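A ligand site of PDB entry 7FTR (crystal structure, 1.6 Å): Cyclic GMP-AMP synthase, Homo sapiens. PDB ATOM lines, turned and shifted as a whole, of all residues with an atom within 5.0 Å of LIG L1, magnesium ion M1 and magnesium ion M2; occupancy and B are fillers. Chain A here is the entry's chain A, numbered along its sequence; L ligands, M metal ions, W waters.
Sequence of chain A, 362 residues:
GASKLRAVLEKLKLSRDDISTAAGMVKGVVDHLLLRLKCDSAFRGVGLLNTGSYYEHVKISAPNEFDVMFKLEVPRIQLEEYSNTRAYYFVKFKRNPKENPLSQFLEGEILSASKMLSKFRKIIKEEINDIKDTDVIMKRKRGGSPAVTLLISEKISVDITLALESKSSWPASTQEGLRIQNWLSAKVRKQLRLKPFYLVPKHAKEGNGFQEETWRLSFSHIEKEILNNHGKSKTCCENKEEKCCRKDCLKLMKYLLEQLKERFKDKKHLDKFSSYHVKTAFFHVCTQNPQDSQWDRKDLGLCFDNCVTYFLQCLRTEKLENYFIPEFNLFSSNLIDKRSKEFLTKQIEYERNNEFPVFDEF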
ATOM      1  N   GLY A  52      17.731 -21.377   3.251  1.00  0.00           N
ATOM      2  CA  GLY A  52      18.640 -20.324   2.821  1.00  0.00           C
ATOM      3  C   GLY A  52      20.065 -20.531   3.256  1.00  0.00           C
ATOM      4  O   GLY A  52      20.427 -21.590   3.791  1.00  0.00           O
ATOM      5  N   SER A  53      20.911 -19.535   2.965  1.00  0.00           N
ATOM      6  CA  SER A  53      22.361 -19.702   3.085  1.00  0.00           C
ATOM      7  C   SER A  53      22.846 -19.951   4.491  1.00  0.00           C
ATOM      8  O   SER A  53      23.810 -20.709   4.661  1.00  0.00           O
ATOM      9  CB  SER A  53      23.104 -18.535   2.459  1.00  0.00           C
ATOM     10  OG  SER A  53      22.739 -17.362   3.152  1.00  0.00           O
ATOM     11  N   GLU A  56      22.399 -23.587   5.151  1.00  0.00           N
ATOM     12  CA  GLU A  56      23.209 -24.342   4.182  1.00  0.00           C
ATOM     13  C   GLU A  56      24.703 -24.123   4.462  1.00  0.00           C
ATOM     14  O   GLU A  56      25.546 -24.697   3.770  1.00  0.00           O
ATOM     15  CB  GLU A  56      22.923 -23.798   2.787  1.00  0.00           C
ATOM     16  CG  GLU A  56      21.541 -24.177   2.303  1.00  0.00           C
ATOM     17  CD  GLU A  56      21.032 -23.366   1.136  1.00  0.00           C
ATOM     18  OE1 GLU A  56      21.626 -22.312   0.838  1.00  0.00           O
ATOM     19  OE2 GLU A  56      20.020 -23.788   0.531  1.00  0.00           O
ATOM     20  N   LYS A  59      26.383 -18.825   4.025  1.00  0.00           N
ATOM     21  CA  LYS A  59      26.207 -17.401   4.355  1.00  0.00           C
ATOM     22  C   LYS A  59      27.613 -16.847   4.516  1.00  0.00           C
ATOM     23  O   LYS A  59      28.474 -17.499   5.114  1.00  0.00           O
ATOM     24  CB  LYS A  59      25.447 -17.249   5.681  1.00  0.00           C
ATOM     25  CG  LYS A  59      25.223 -15.802   6.118  1.00  0.00           C
ATOM     26  CD  LYS A  59      24.142 -15.124   5.298  1.00  0.00           C
ATOM     27  CE  LYS A  59      23.978 -13.634   5.543  1.00  0.00           C
ATOM     28  NZ  LYS A  59      25.199 -12.840   5.172  1.00  0.00           N
ATOM     29  N   GLU A  65      21.342 -12.454   8.005  1.00  0.00           N
ATOM     30  CA  GLU A  65      20.146 -12.657   7.191  1.00  0.00           C
ATOM     31  C   GLU A  65      19.804 -14.136   7.212  1.00  0.00           C
ATOM     32  O   GLU A  65      20.614 -14.981   6.820  1.00  0.00           O
ATOM     33  CB  GLU A  65      20.281 -12.074   5.767  1.00  0.00           C
ATOM     34  CG  GLU A  65      18.950 -11.866   5.052  1.00  0.00           C
ATOM     35  CD  GLU A  65      18.538 -12.971   4.094  1.00  0.00           C
ATOM     36  OE1 GLU A  65      19.237 -13.993   4.003  1.00  0.00           O
ATOM     37  OE2 GLU A  65      17.498 -12.809   3.421  1.00  0.00           O
ATOM     38  N   ASP A  67      16.632 -17.024   6.650  1.00  0.00           N
ATOM     39  CA  ASP A  67      15.437 -17.307   5.877  1.00  0.00           C
ATOM     40  C   ASP A  67      14.730 -18.457   6.531  1.00  0.00           C
ATOM     41  O   ASP A  67      15.349 -19.446   6.961  1.00  0.00           O
ATOM     42  CB  ASP A  67      15.795 -17.606   4.427  1.00  0.00           C
ATOM     43  CG  ASP A  67      16.579 -16.469   3.802  1.00  0.00           C
ATOM     44  OD1 ASP A  67      15.945 -15.450   3.430  1.00  0.00           O
ATOM     45  OD2 ASP A  67      17.849 -16.626   3.644  1.00  0.00           O
ATOM     46  N   ASP A 159      13.827 -13.194   6.922  1.00  0.00           N
ATOM     47  CA  ASP A 159      12.830 -13.287   5.868  1.00  0.00           C
ATOM     48  C   ASP A 159      11.957 -14.467   6.163  1.00  0.00           C
ATOM     49  O   ASP A 159      12.446 -15.608   6.241  1.00  0.00           O
ATOM     50  CB  ASP A 159      13.467 -13.439   4.465  1.00  0.00           C
ATOM     51  CG  ASP A 159      14.118 -12.218   3.892  1.00  0.00           C
ATOM     52  OD1 ASP A 159      13.828 -11.099   4.376  1.00  0.00           O
ATOM     53  OD2 ASP A 159      14.877 -12.364   2.926  1.00  0.00           O
ATOM     54  N   ARG A 216       4.276 -19.421  -6.448  1.00  0.00           N
ATOM     55  CA  ARG A 216       5.414 -20.009  -7.167  1.00  0.00           C
ATOM     56  C   ARG A 216       5.987 -21.204  -6.431  1.00  0.00           C
ATOM     57  O   ARG A 216       6.011 -21.211  -5.192  1.00  0.00           O
ATOM     58  CB  ARG A 216       6.535 -18.974  -7.419  1.00  0.00           C
ATOM     59  CG  ARG A 216       7.521 -19.438  -8.522  1.00  0.00           C
ATOM     60  CD  ARG A 216       8.915 -18.904  -8.360  1.00  0.00           C
ATOM     61  NE  ARG A 216       9.493 -19.513  -7.157  1.00  0.00           N
ATOM     62  CZ  ARG A 216      10.001 -18.837  -6.135  1.00  0.00           C
ATOM     63  NH1 ARG A 216      10.392 -19.484  -5.044  1.00  0.00           N
ATOM     64  NH2 ARG A 216      10.152 -17.516  -6.204  1.00  0.00           N
ATOM     65  N   LEU A 217       6.488 -22.199  -7.202  1.00  0.00           N
ATOM     66  CA  LEU A 217       7.121 -23.383  -6.628  1.00  0.00           C
ATOM     67  C   LEU A 217       8.390 -23.007  -5.886  1.00  0.00           C
ATOM     68  O   LEU A 217       9.160 -22.152  -6.336  1.00  0.00           O
ATOM     69  CB  LEU A 217       7.432 -24.482  -7.674  1.00  0.00           C
ATOM     70  CG  LEU A 217       6.238 -25.174  -8.358  1.00  0.00           C
ATOM     71  CD1 LEU A 217       6.708 -26.179  -9.412  1.00  0.00           C
ATOM     72  CD2 LEU A 217       5.369 -25.898  -7.351  1.00  0.00           C
ATOM     73  N   SER A 220      13.348 -24.832  -1.616  1.00  0.00           N
ATOM     74  CA  SER A 220      14.369 -24.393  -0.631  1.00  0.00           C
ATOM     75  C   SER A 220      14.833 -25.530   0.290  1.00  0.00           C
ATOM     76  O   SER A 220      16.019 -25.590   0.654  1.00  0.00           O
ATOM     77  CB  SER A 220      13.789 -23.275   0.232  1.00  0.00           C
ATOM     78  OG  SER A 220      13.437 -22.159  -0.559  1.00  0.00           O
ATOM     79  N   GLU A 223      17.150 -27.725  -1.739  1.00  0.00           N
ATOM     80  CA  GLU A 223      18.426 -27.031  -1.943  1.00  0.00           C
ATOM     81  C   GLU A 223      19.275 -27.147  -0.684  1.00  0.00           C
ATOM     82  O   GLU A 223      20.467 -27.379  -0.781  1.00  0.00           O
ATOM     83  CB  GLU A 223      18.186 -25.547  -2.274  1.00  0.00           C
ATOM     84  CG  GLU A 223      17.457 -25.372  -3.596  1.00  0.00           C
ATOM     85  CD  GLU A 223      16.897 -23.983  -3.860  1.00  0.00           C
ATOM     86  OE1 GLU A 223      17.314 -23.047  -3.142  1.00  0.00           O
ATOM     87  OE2 GLU A 223      16.076 -23.819  -4.777  1.00  0.00           O
ATOM     88  N   LYS A 254      29.121 -15.867  -4.606  1.00  0.00           N
ATOM     89  CA  LYS A 254      28.211 -14.941  -3.918  1.00  0.00           C
ATOM     90  C   LYS A 254      28.910 -13.631  -3.630  1.00  0.00           C
ATOM     91  O   LYS A 254      28.299 -12.576  -3.789  1.00  0.00           O
ATOM     92  CB  LYS A 254      27.726 -15.553  -2.578  1.00  0.00           C
ATOM     93  CG  LYS A 254      26.865 -16.795  -2.776  1.00  0.00           C
ATOM     94  CD  LYS A 254      26.563 -17.552  -1.464  1.00  0.00           C
ATOM     95  CE  LYS A 254      25.939 -16.687  -0.377  1.00  0.00           C
ATOM     96  NZ  LYS A 254      24.615 -16.164  -0.827  1.00  0.00           N
ATOM     97  N   GLU A 258      28.018  -9.842  -4.790  1.00  0.00           N
ATOM     98  CA  GLU A 258      27.735  -8.846  -3.759  1.00  0.00           C
ATOM     99  C   GLU A 258      28.668  -7.622  -3.931  1.00  0.00           C
ATOM    100  O   GLU A 258      28.214  -6.462  -3.816  1.00  0.00           O
ATOM    101  CB  GLU A 258      27.928  -9.433  -2.339  1.00  0.00           C
ATOM    102  CG  GLU A 258      26.861 -10.393  -1.839  1.00  0.00           C
ATOM    103  CD  GLU A 258      26.950 -10.747  -0.360  1.00  0.00           C
ATOM    104  OE1 GLU A 258      27.682 -10.040   0.372  1.00  0.00           O
ATOM    105  OE2 GLU A 258      26.290 -11.722   0.069  1.00  0.00           O
ATOM    106  N   SER A 275      21.599 -13.363  -5.326  1.00  0.00           N
ATOM    107  CA  SER A 275      22.443 -14.510  -4.950  1.00  0.00           C
ATOM    108  C   SER A 275      21.819 -15.797  -5.465  1.00  0.00           C
ATOM    109  O   SER A 275      22.537 -16.753  -5.698  1.00  0.00           O
ATOM    110  CB  SER A 275      22.601 -14.574  -3.429  1.00  0.00           C
ATOM    111  OG  SER A 275      21.331 -14.757  -2.836  1.00  0.00           O
ATOM    112  N   TYR A 276      20.471 -15.850  -5.605  1.00  0.00           N
ATOM    113  CA  TYR A 276      19.814 -17.056  -6.162  1.00  0.00           C
ATOM    114  C   TYR A 276      20.261 -17.400  -7.601  1.00  0.00           C
ATOM    115  O   TYR A 276      20.297 -18.582  -7.974  1.00  0.00           O
ATOM    116  CB  TYR A 276      18.280 -16.991  -6.104  1.00  0.00           C
ATOM    117  CG  TYR A 276      17.642 -18.354  -6.297  1.00  0.00           C
ATOM    118  CD1 TYR A 276      17.862 -19.390  -5.376  1.00  0.00           C
ATOM    119  CD2 TYR A 276      16.896 -18.645  -7.436  1.00  0.00           C
ATOM    120  CE1 TYR A 276      17.342 -20.668  -5.595  1.00  0.00           C
ATOM    121  CE2 TYR A 276      16.375 -19.923  -7.654  1.00  0.00           C
ATOM    122  CZ  TYR A 276      16.540 -20.909  -6.698  1.00  0.00           C
ATOM    123  OH  TYR A 276      16.017 -22.153  -6.928  1.00  0.00           O
ATOM    124  N   LYS A 279      23.518 -19.157  -6.982  1.00  0.00           N
ATOM    125  CA  LYS A 279      23.260 -20.457  -6.378  1.00  0.00           C
ATOM    126  C   LYS A 279      22.778 -21.433  -7.446  1.00  0.00           C
ATOM    127  O   LYS A 279      23.262 -22.571  -7.500  1.00  0.00           O
ATOM    128  CB  LYS A 279      22.210 -20.298  -5.278  1.00  0.00           C
ATOM    129  CG  LYS A 279      22.101 -21.551  -4.404  1.00  0.00           C
ATOM    130  CD  LYS A 279      20.870 -21.369  -3.490  1.00  0.00           C
ATOM    131  CE  LYS A 279      20.838 -22.443  -2.438  1.00  0.00           C
ATOM    132  NZ  LYS A 279      19.585 -22.314  -1.656  1.00  0.00           N
ATOM    133  N   ASN A 322      15.963 -22.656 -13.886  1.00  0.00           N
ATOM    134  CA  ASN A 322      15.732 -22.937 -12.471  1.00  0.00           C
ATOM    135  C   ASN A 322      16.139 -24.444 -12.372  1.00  0.00           C
ATOM    136  O   ASN A 322      15.824 -25.243 -13.257  1.00  0.00           O
ATOM    137  CB  ASN A 322      14.245 -22.729 -12.147  1.00  0.00           C
ATOM    138  CG  ASN A 322      13.823 -23.240 -10.786  1.00  0.00           C
ATOM    139  OD1 ASN A 322      13.824 -24.436 -10.505  1.00  0.00           O
ATOM    140  ND2 ASN A 322      13.423 -22.327  -9.919  1.00  0.00           N
ATOM    141  N   LEU A 330      15.446 -18.061 -15.581  1.00  0.00           N
ATOM    142  CA  LEU A 330      15.705 -16.931 -14.695  1.00  0.00           C
ATOM    143  C   LEU A 330      16.350 -15.743 -15.443  1.00  0.00           C
ATOM    144  O   LEU A 330      16.245 -14.602 -14.969  1.00  0.00           O
ATOM    145  CB  LEU A 330      16.639 -17.356 -13.524  1.00  0.00           C
ATOM    146  CG  LEU A 330      16.208 -18.586 -12.659  1.00  0.00           C
ATOM    147  CD1 LEU A 330      17.215 -18.858 -11.604  1.00  0.00           C
ATOM    148  CD2 LEU A 330      14.915 -18.326 -11.969  1.00  0.00           C
HETATM  149  P1  LIG L   1      21.918 -14.954   0.865  1.00  0.00           P
HETATM  150  O1  LIG L   1      20.825 -14.657   1.866  1.00  0.00           O
HETATM  151  O2  LIG L   1      22.129 -13.981  -0.257  1.00  0.00           O
HETATM  152  O3  LIG L   1      23.254 -15.250   1.463  1.00  0.00           O
HETATM  153  P2  LIG L   1      20.115 -17.123   0.249  1.00  0.00           P
HETATM  154  O4  LIG L   1      20.189 -18.444  -0.446  1.00  0.00           O
HETATM  155  O5  LIG L   1      19.600 -17.308   1.676  1.00  0.00           O
HETATM  156  O6  LIG L   1      21.494 -16.343   0.230  1.00  0.00           O
HETATM  157  P3  LIG L   1      17.685 -15.502  -0.221  1.00  0.00           P
HETATM  158  O7  LIG L   1      17.553 -14.347  -1.143  1.00  0.00           O
HETATM  159  O8  LIG L   1      17.865 -15.085   1.222  1.00  0.00           O
HETATM  160  O9  LIG L   1      19.081 -16.200  -0.544  1.00  0.00           O
HETATM  161  O10 LIG L   1      16.578 -16.596  -0.337  1.00  0.00           O
HETATM  162  C1  LIG L   1      16.402 -17.678   0.570  1.00  0.00           C
HETATM  163  C2  LIG L   1      16.022 -18.880  -0.250  1.00  0.00           C
HETATM  164  O11 LIG L   1      14.836 -18.575  -1.006  1.00  0.00           O
HETATM  165  C3  LIG L   1      17.030 -19.304  -1.313  1.00  0.00           C
HETATM  166  O12 LIG L   1      18.093 -20.075  -0.756  1.00  0.00           O
HETATM  167  C4  LIG L   1      16.158 -20.114  -2.258  1.00  0.00           C
HETATM  168  O13 LIG L   1      15.907 -21.401  -1.714  1.00  0.00           O
HETATM  169  C5  LIG L   1      14.840 -19.301  -2.222  1.00  0.00           C
HETATM  170  N1  LIG L   1      14.706 -18.357  -3.321  1.00  0.00           N
HETATM  171  C6  LIG L   1      15.155 -17.059  -3.385  1.00  0.00           C
HETATM  172  N2  LIG L   1      14.986 -16.488  -4.555  1.00  0.00           N
HETATM  173  C7  LIG L   1      14.359 -17.466  -5.311  1.00  0.00           C
HETATM  174  C8  LIG L   1      13.877 -17.484  -6.631  1.00  0.00           C
HETATM  175  N3  LIG L   1      13.991 -16.448  -7.472  1.00  0.00           N
HETATM  176  N4  LIG L   1      13.330 -18.629  -7.082  1.00  0.00           N
HETATM  177  C9  LIG L   1      13.255 -19.685  -6.272  1.00  0.00           C
HETATM  178  N5  LIG L   1      13.653 -19.784  -4.992  1.00  0.00           N
HETATM  179  C10 LIG L   1      14.188 -18.628  -4.569  1.00  0.00           C
HETATM  180  C1  LG2 L   2      11.728 -16.719  -2.673  1.00  0.00           C
HETATM  181  C2  LG2 L   2      11.335 -18.916  -1.619  1.00  0.00           C
HETATM  182  C3  LG2 L   2      12.196 -14.398  -3.541  1.00  0.00           C
HETATM  183  C4  LG2 L   2      12.143 -14.617  -4.918  1.00  0.00           C
HETATM  184  C5  LG2 L   2      12.305 -13.086  -3.071  1.00  0.00           C
HETATM  185  C6  LG2 L   2      12.162 -13.548  -5.806  1.00  0.00           C
HETATM  186  C7  LG2 L   2      12.333 -12.018  -3.962  1.00  0.00           C
HETATM  187  C8  LG2 L   2      12.246 -12.236  -5.340  1.00  0.00           C
HETATM  188  C9  LG2 L   2      12.280 -11.093  -6.307  1.00  0.00           C
HETATM  189  C10 LG2 L   2      12.364  -9.688  -5.790  1.00  0.00           C
HETATM  190  C11 LG2 L   2      12.371 -18.032   0.975  1.00  0.00           C
HETATM  191  C12 LG2 L   2      12.247 -17.188  -0.226  1.00  0.00           C
HETATM  192  C13 LG2 L   2      12.486 -17.695   2.294  1.00  0.00           C
HETATM  193  C14 LG2 L   2      12.457 -19.442   0.977  1.00  0.00           C
HETATM  194  C15 LG2 L   2      11.807 -17.569  -1.473  1.00  0.00           C
HETATM  195  O1  LG2 L   2      12.712 -15.964  -0.045  1.00  0.00           O
HETATM  196  O2  LG2 L   2      12.625 -18.811   3.027  1.00  0.00           O
HETATM  197  C16 LG2 L   2      12.498 -16.420   3.042  1.00  0.00           C
HETATM  198  N1  LG2 L   2      12.601 -19.930   2.171  1.00  0.00           N
HETATM  199  N2  LG2 L   2      12.184 -15.434  -2.574  1.00  0.00           N
HETATM  200  O3  LG2 L   2      11.302 -17.188  -3.727  1.00  0.00           O
HETATM  201  N3  LG2 L   2      10.912 -19.959  -1.771  1.00  0.00           N
HETATM  202  O4  LG2 L   2      12.226 -11.296  -7.521  1.00  0.00           O
HETATM  203 MG    MG M   1      19.265 -15.613   2.785  1.00  0.00          MG
HETATM  204 MG    MG M   2      16.221 -13.821   2.117  1.00  0.00          MG
HETATM  205  O   HOH W   1      23.362 -11.253  -0.331  1.00  0.00           O
HETATM  206  O   HOH W   2      15.487 -12.825  -1.834  1.00  0.00           O
HETATM  207  O   HOH W   3      18.510 -14.278  -3.704  1.00  0.00           O
HETATM  208  O   HOH W   4      16.770 -12.371   0.958  1.00  0.00           O
HETATM  209  O   HOH W   5      13.446 -23.017  -4.762  1.00  0.00           O
HETATM  210  O   HOH W   6      25.464 -14.245   2.277  1.00  0.00           O
HETATM  211  O   HOH W   7      20.796 -17.618  -3.040  1.00  0.00           O
HETATM  212  O   HOH W   8      12.858 -19.673  -9.614  1.00  0.00           O
HETATM  213  O   HOH W   9      20.616 -16.180   4.320  1.00  0.00           O
HETATM  214  O   HOH W  10      22.427 -20.156  -0.621  1.00  0.00           O
HETATM  215  O   HOH W  11      19.375 -12.443  -1.249  1.00  0.00           O
HETATM  216  O   HOH W  12      25.125 -13.500  -1.530  1.00  0.00           O
HETATM  217  O   HOH W  13      15.890 -13.855  -7.897  1.00  0.00           O
HETATM  218  O   HOH W  14      13.819 -15.172 -10.661  1.00  0.00           O
HETATM  219  O   HOH W  15      14.515 -14.425   1.018  1.00  0.00           O
HETATM  220  O   HOH W  16      15.944 -13.966  -4.632  1.00  0.00           O
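Three residues have an atom within 4 Å of magnesium ion M2: Glu 65, Asp 67 and Asp 159.
Residues that only touch LIG L1: Tyr 276 (3.3 Å), Gly 52 (3.4 Å) and Lys 59 (3.9 Å).
12 residues have an atom within 4 Å of LIG L1: Gly 52, Ser 53, Lys 59, Glu 65, Asp 67, Arg 216, Ser 220, Glu 223, Lys 254, Ser 275, Tyr 276 and Lys 279.
O13 of LIG L1 lies within hydrogen-bond range of OE1 of Glu 223 (2.6 Å).
N of Ser 53 sits close to O5 of LIG L1, 2.9 Å away.
OG of Ser 53 lies within hydrogen-bond range of O3 of LIG L1.
OG of Ser 275 lies within hydrogen-bond range of O2 of LIG L1, 2.8 Å away.
The side-chain amino group of Lys 254 lies within salt-bridge range of an oxygen (O3) of LIG L1.
OG of Ser 220 sits at hydrogen-bond distance from O13 of LIG L1 (2.8 Å).
The side-chain amino group (NZ) of Lys 279 sits at hydrogen-bond distance from an oxygen (O12) of LIG L1, 2.8 Å away.
The guanidinium group (NH1) of Arg 216 sits close to a nitrogen (N5) of LIG L1.
The guanidinium group (NH2) of Arg 216 is in hydrogen-bond range of an oxygen (O3) of LG2 L2, 2.8 Å away.
Water W15 bridges O1 of LG2 L2 (2.6 Å) and O10 of LIG L1 (3.3 Å).
Water W6 lies within hydrogen-bond range of O3 of LIG L1 (2.6 Å), NZ of Lys 59 (3.2 Å) and OE2 of Glu 258 (3.5 Å).
Water W11 bridges O7 of LIG L1 and OG of Ser 275.
Water W10 bridges OE1 of Glu 56 (2.7 Å) and O4 of LIG L1 (2.8 Å).
Water W1 lies within hydrogen-bond range of the side-chain carboxylate (OE2) of Glu 258 (3.0 Å) and an oxygen (O2) of LIG L1 (3.0 Å).
Water W5 lies within hydrogen-bond range of OE2 of Glu 223, N5 of LIG L1 and OH of Tyr 276.
Merely in contact with magnesium ion M1: Ser 53.
Of the 18 residues printed, 3 come within 4 Å of magnesium ion M1.
Water W4 binds magnesium ion M2 (1.9 Å).
The side-chain carboxylate (OE2) of Glu 65 binds magnesium ion M2.
Magnesium ion M2 is bound by OD1 of Asp 67, 2.1 Å away.
Magnesium ion M2 is bound by water W15 (2.1 Å).
OD2 of Asp 159 is bound to magnesium ion M2 (2.1 Å).
Magnesium ion M2 is bound by an oxygen (O8) of LIG L1.
Magnesium ion M2 has six donor atoms within binding distance.
Magnesium ion M1 is bound by OD2 of Asp 67, 1.9 Å away.
Magnesium ion M1 is bound by OE1 of Glu 65.
O1 of LIG L1 binds magnesium ion M1 (2.0 Å).
An oxygen (O5) of LIG L1 is bound to magnesium ion M1 (2.1 Å).
Magnesium ion M1 is bound by water W9 (2.1 Å).
O8 of LIG L1 is bound to magnesium ion M1 (2.2 Å).
Magnesium ion M1 has six donor atoms within binding distance.
O1 of LG2 L2 sits close to O11 of LIG L1, 3.5 Å away.
The side-chain carboxylate of Glu 223 is in salt-bridge range of the side-chain amino group of Lys 279 (2.8 Å).
The side-chain carboxylate (OE2) of Glu 223 sits at hydrogen-bond distance from the side-chain hydroxyl (OH) of Tyr 276, at 2.7 Å.
O of Ser 53 lies within hydrogen-bond range of N of Lys 59, at 3.3 Å.
The side-chain carboxylate of Glu 56 lies within salt-bridge range of the side-chain amino group of Lys 279, 2.7 Å away.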
